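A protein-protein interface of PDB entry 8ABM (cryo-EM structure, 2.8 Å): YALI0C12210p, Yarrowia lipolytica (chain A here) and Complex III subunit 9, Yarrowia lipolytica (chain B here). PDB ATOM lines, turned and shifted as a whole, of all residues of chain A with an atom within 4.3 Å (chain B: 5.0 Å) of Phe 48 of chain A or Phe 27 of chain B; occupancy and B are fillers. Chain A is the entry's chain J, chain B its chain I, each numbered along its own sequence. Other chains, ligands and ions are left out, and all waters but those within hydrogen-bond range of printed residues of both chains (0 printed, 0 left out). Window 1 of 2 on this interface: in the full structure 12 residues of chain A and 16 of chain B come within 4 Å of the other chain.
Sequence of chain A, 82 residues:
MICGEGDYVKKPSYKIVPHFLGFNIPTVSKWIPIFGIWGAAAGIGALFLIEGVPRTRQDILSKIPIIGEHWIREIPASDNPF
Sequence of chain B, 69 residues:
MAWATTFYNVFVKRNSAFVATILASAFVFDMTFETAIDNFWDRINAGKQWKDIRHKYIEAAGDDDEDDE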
ATOM      1  N   ILE A  44     -29.037  11.711  30.692  1.00  0.00           N
ATOM      2  CA  ILE A  44     -28.016  11.153  29.818  1.00  0.00           C
ATOM      3  C   ILE A  44     -27.380   9.961  30.528  1.00  0.00           C
ATOM      4  O   ILE A  44     -27.266   8.895  29.934  1.00  0.00           O
ATOM      5  CB  ILE A  44     -26.981  12.229  29.413  1.00  0.00           C
ATOM      6  CG1 ILE A  44     -27.578  13.259  28.447  1.00  0.00           C
ATOM      7  CG2 ILE A  44     -25.706  11.615  28.842  1.00  0.00           C
ATOM      8  CD1 ILE A  44     -26.895  14.619  28.471  1.00  0.00           C
ATOM      9  N   GLY A  45     -27.016  10.147  31.804  1.00  0.00           N
ATOM     10  CA  GLY A  45     -26.320   9.127  32.574  1.00  0.00           C
ATOM     11  C   GLY A  45     -27.172   7.881  32.792  1.00  0.00           C
ATOM     12  O   GLY A  45     -26.687   6.760  32.635  1.00  0.00           O
ATOM     13  N   ALA A  46     -28.449   8.101  33.139  1.00  0.00           N
ATOM     14  CA  ALA A  46     -29.353   7.000  33.428  1.00  0.00           C
ATOM     15  C   ALA A  46     -29.569   6.190  32.157  1.00  0.00           C
ATOM     16  O   ALA A  46     -29.447   4.967  32.169  1.00  0.00           O
ATOM     17  CB  ALA A  46     -30.659   7.504  33.995  1.00  0.00           C
ATOM     18  N   LEU A  47     -29.829   6.907  31.063  1.00  0.00           N
ATOM     19  CA  LEU A  47     -30.161   6.287  29.796  1.00  0.00           C
ATOM     20  C   LEU A  47     -28.960   5.495  29.290  1.00  0.00           C
ATOM     21  O   LEU A  47     -29.119   4.411  28.734  1.00  0.00           O
ATOM     22  CB  LEU A  47     -30.568   7.379  28.807  1.00  0.00           C
ATOM     23  CG  LEU A  47     -30.897   6.882  27.403  1.00  0.00           C
ATOM     24  CD1 LEU A  47     -32.216   6.120  27.391  1.00  0.00           C
ATOM     25  CD2 LEU A  47     -30.944   8.043  26.427  1.00  0.00           C
ATOM     26  N   PHE A  48     -27.770   6.057  29.515  1.00  0.00           N
ATOM     27  CA  PHE A  48     -26.500   5.434  29.198  1.00  0.00           C
ATOM     28  C   PHE A  48     -26.343   4.116  29.950  1.00  0.00           C
ATOM     29  O   PHE A  48     -25.868   3.141  29.374  1.00  0.00           O
ATOM     30  CB  PHE A  48     -25.364   6.404  29.528  1.00  0.00           C
ATOM     31  CG  PHE A  48     -23.981   5.921  29.177  1.00  0.00           C
ATOM     32  CD1 PHE A  48     -23.728   5.234  27.992  1.00  0.00           C
ATOM     33  CD2 PHE A  48     -22.914   6.188  30.023  1.00  0.00           C
ATOM     34  CE1 PHE A  48     -22.446   4.800  27.675  1.00  0.00           C
ATOM     35  CE2 PHE A  48     -21.630   5.765  29.701  1.00  0.00           C
ATOM     36  CZ  PHE A  48     -21.397   5.070  28.529  1.00  0.00           C
ATOM     37  N   LEU A  49     -26.742   4.098  31.227  1.00  0.00           N
ATOM     38  CA  LEU A  49     -26.592   2.912  32.054  1.00  0.00           C
ATOM     39  C   LEU A  49     -27.517   1.792  31.597  1.00  0.00           C
ATOM     40  O   LEU A  49     -27.215   0.620  31.817  1.00  0.00           O
ATOM     41  CB  LEU A  49     -26.896   3.255  33.512  1.00  0.00           C
ATOM     42  CG  LEU A  49     -25.710   3.732  34.338  1.00  0.00           C
ATOM     43  CD1 LEU A  49     -26.189   4.157  35.715  1.00  0.00           C
ATOM     44  CD2 LEU A  49     -24.657   2.640  34.458  1.00  0.00           C
ATOM     45  N   ILE A  50     -28.666   2.143  31.019  1.00  0.00           N
ATOM     46  CA  ILE A  50     -29.605   1.088  30.668  1.00  0.00           C
ATOM     47  C   ILE A  50     -29.673   0.913  29.158  1.00  0.00           C
ATOM     48  O   ILE A  50     -30.630   0.342  28.645  1.00  0.00           O
ATOM     49  CB  ILE A  50     -30.994   1.338  31.272  1.00  0.00           C
ATOM     50  CG1 ILE A  50     -31.566   2.673  30.784  1.00  0.00           C
ATOM     51  CG2 ILE A  50     -30.936   1.212  32.790  1.00  0.00           C
ATOM     52  CD1 ILE A  50     -33.054   2.817  30.963  1.00  0.00           C
ATOM     53  N   GLU A  51     -28.652   1.402  28.458  1.00  0.00           N
ATOM     54  CA  GLU A  51     -28.616   1.343  27.010  1.00  0.00           C
ATOM     55  C   GLU A  51     -28.667  -0.123  26.585  1.00  0.00           C
ATOM     56  O   GLU A  51     -29.167  -0.448  25.516  1.00  0.00           O
ATOM     57  CB  GLU A  51     -27.346   2.056  26.543  1.00  0.00           C
ATOM     58  CG  GLU A  51     -27.033   1.914  25.055  1.00  0.00           C
ATOM     59  CD  GLU A  51     -26.354   0.640  24.561  1.00  0.00           C
ATOM     60  OE1 GLU A  51     -25.534   0.060  25.313  1.00  0.00           O
ATOM     61  OE2 GLU A  51     -26.631   0.231  23.409  1.00  0.00           O
ATOM     62  N   LEU B  23     -20.479  12.760  30.213  1.00  0.00           N
ATOM     63  CA  LEU B  23     -21.354  11.609  30.055  1.00  0.00           C
ATOM     64  C   LEU B  23     -21.863  11.500  28.627  1.00  0.00           C
ATOM     65  O   LEU B  23     -21.966  10.386  28.133  1.00  0.00           O
ATOM     66  CB  LEU B  23     -22.518  11.645  31.044  1.00  0.00           C
ATOM     67  CG  LEU B  23     -22.085  11.605  32.503  1.00  0.00           C
ATOM     68  CD1 LEU B  23     -23.275  11.778  33.428  1.00  0.00           C
ATOM     69  CD2 LEU B  23     -21.321  10.331  32.812  1.00  0.00           C
ATOM     70  N   ALA B  24     -22.158  12.628  27.969  1.00  0.00           N
ATOM     71  CA  ALA B  24     -22.590  12.564  26.579  1.00  0.00           C
ATOM     72  C   ALA B  24     -21.451  12.059  25.690  1.00  0.00           C
ATOM     73  O   ALA B  24     -21.677  11.274  24.770  1.00  0.00           O
ATOM     74  CB  ALA B  24     -23.113  13.901  26.123  1.00  0.00           C
ATOM     75  N   SER B  25     -20.225  12.494  25.989  1.00  0.00           N
ATOM     76  CA  SER B  25     -19.050  12.028  25.271  1.00  0.00           C
ATOM     77  C   SER B  25     -18.853  10.534  25.492  1.00  0.00           C
ATOM     78  O   SER B  25     -18.457   9.831  24.573  1.00  0.00           O
ATOM     79  CB  SER B  25     -17.832  12.777  25.707  1.00  0.00           C
ATOM     80  OG  SER B  25     -17.986  14.154  25.433  1.00  0.00           O
ATOM     81  N   ALA B  26     -19.083  10.084  26.732  1.00  0.00           N
ATOM     82  CA  ALA B  26     -18.915   8.690  27.100  1.00  0.00           C
ATOM     83  C   ALA B  26     -19.890   7.847  26.294  1.00  0.00           C
ATOM     84  O   ALA B  26     -19.516   6.780  25.831  1.00  0.00           O
ATOM     85  CB  ALA B  26     -19.101   8.489  28.585  1.00  0.00           C
ATOM     86  N   PHE B  27     -21.125   8.337  26.154  1.00  0.00           N
ATOM     87  CA  PHE B  27     -22.155   7.649  25.400  1.00  0.00           C
ATOM     88  C   PHE B  27     -21.695   7.499  23.957  1.00  0.00           C
ATOM     89  O   PHE B  27     -21.745   6.403  23.414  1.00  0.00           O
ATOM     90  CB  PHE B  27     -23.474   8.417  25.467  1.00  0.00           C
ATOM     91  CG  PHE B  27     -24.718   7.569  25.380  1.00  0.00           C
ATOM     92  CD1 PHE B  27     -24.751   6.381  24.656  1.00  0.00           C
ATOM     93  CD2 PHE B  27     -25.880   7.979  26.018  1.00  0.00           C
ATOM     94  CE1 PHE B  27     -25.903   5.611  24.591  1.00  0.00           C
ATOM     95  CE2 PHE B  27     -27.037   7.215  25.946  1.00  0.00           C
ATOM     96  CZ  PHE B  27     -27.047   6.034  25.234  1.00  0.00           C
ATOM     97  N   VAL B  28     -21.196   8.584  23.371  1.00  0.00           N
ATOM     98  CA  VAL B  28     -20.828   8.557  21.968  1.00  0.00           C
ATOM     99  C   VAL B  28     -19.608   7.663  21.782  1.00  0.00           C
ATOM    100  O   VAL B  28     -19.571   6.852  20.862  1.00  0.00           O
ATOM    101  CB  VAL B  28     -20.584   9.976  21.435  1.00  0.00           C
ATOM    102  CG1 VAL B  28     -19.874   9.959  20.094  1.00  0.00           C
ATOM    103  CG2 VAL B  28     -21.880  10.754  21.352  1.00  0.00           C
ATOM    104  N   PHE B  29     -18.624   7.808  22.667  1.00  0.00           N
ATOM    105  CA  PHE B  29     -17.433   6.989  22.577  1.00  0.00           C
ATOM    106  C   PHE B  29     -17.823   5.516  22.662  1.00  0.00           C
ATOM    107  O   PHE B  29     -17.456   4.729  21.800  1.00  0.00           O
ATOM    108  CB  PHE B  29     -16.457   7.342  23.694  1.00  0.00           C
ATOM    109  CG  PHE B  29     -15.299   6.388  23.756  1.00  0.00           C
ATOM    110  CD1 PHE B  29     -14.230   6.528  22.881  1.00  0.00           C
ATOM    111  CD2 PHE B  29     -15.294   5.325  24.650  1.00  0.00           C
ATOM    112  CE1 PHE B  29     -13.161   5.643  22.922  1.00  0.00           C
ATOM    113  CE2 PHE B  29     -14.227   4.436  24.688  1.00  0.00           C
ATOM    114  CZ  PHE B  29     -13.163   4.596  23.823  1.00  0.00           C
ATOM    115  N   ASP B  30     -18.598   5.164  23.689  1.00  0.00           N
ATOM    116  CA  ASP B  30     -19.046   3.795  23.887  1.00  0.00           C
ATOM    117  C   ASP B  30     -19.638   3.202  22.607  1.00  0.00           C
ATOM    118  O   ASP B  30     -19.339   2.059  22.282  1.00  0.00           O
ATOM    119  CB  ASP B  30     -20.049   3.714  25.035  1.00  0.00           C
ATOM    120  CG  ASP B  30     -20.125   2.342  25.686  1.00  0.00           C
ATOM    121  OD1 ASP B  30     -19.180   1.996  26.436  1.00  0.00           O
ATOM    122  OD2 ASP B  30     -21.127   1.629  25.455  1.00  0.00           O
ATOM    123  N   MET B  31     -20.495   3.961  21.911  1.00  0.00           N
ATOM    124  CA  MET B  31     -21.232   3.462  20.758  1.00  0.00           C
ATOM    125  C   MET B  31     -20.314   3.293  19.552  1.00  0.00           C
ATOM    126  O   MET B  31     -20.409   2.313  18.812  1.00  0.00           O
ATOM    127  CB  MET B  31     -22.376   4.411  20.386  1.00  0.00           C
ATOM    128  CG  MET B  31     -23.528   4.389  21.369  1.00  0.00           C
ATOM    129  SD  MET B  31     -24.058   2.709  21.795  1.00  0.00           S
ATOM    130  CE  MET B  31     -23.315   2.533  23.415  1.00  0.00           C
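Among the printed residues, merely in contact across the chains: Ile 44 of chain A with Leu 23 of chain B (3.9 Å), Ile 44 of chain A with Ala 24 of chain B (3.8 Å), Phe 48 of chain A with Ala 26 of chain B (3.7 Å), Phe 48 of chain A with Phe 27 of chain B (3.6 Å), Phe 48 of chain A with Asp 30 of chain B (3.7 Å), Glu 51 of chain A with Phe 27 of chain B (3.9 Å) and Glu 51 of chain A with Met 31 of chain B (3.8 Å).
Of the printed residues of chain B, Ile 44 of chain A touches Leu 23 (3.9 Å) and Ala 24 (3.8 Å).
Leu 47 of chain A touches none of the printed residues of chain B.
Printed residues of chain B within 4 Å of Phe 48 of chain A: Ala 26, Phe 27 and Asp 30.
Leu 49 of chain A touches none of the printed residues of chain B.
Of the printed residues of chain B, Glu 51 of chain A touches Phe 27 and Met 31.
Of the printed residues of chain A, Ala 26 of chain B touches Phe 48 (3.7 Å).
Of chain A, only Phe 48 and Glu 51 come within 4 Å of Phe 27 of chain B.
The nearest residue of chain B that does not touch Phe 48 of chain A is Leu 23 of chain B (4.7 Å).
Of the 9 printed residues of chain B, 6 touch a printed residue of chain A.
Along chain B the printed residues that touch a printed residue of chain A span positions 23 to 31.
Of the 8 printed residues of chain A, 3 touch a printed residue of chain B.
Among the printed residues, 7 pairs touch across the chains.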
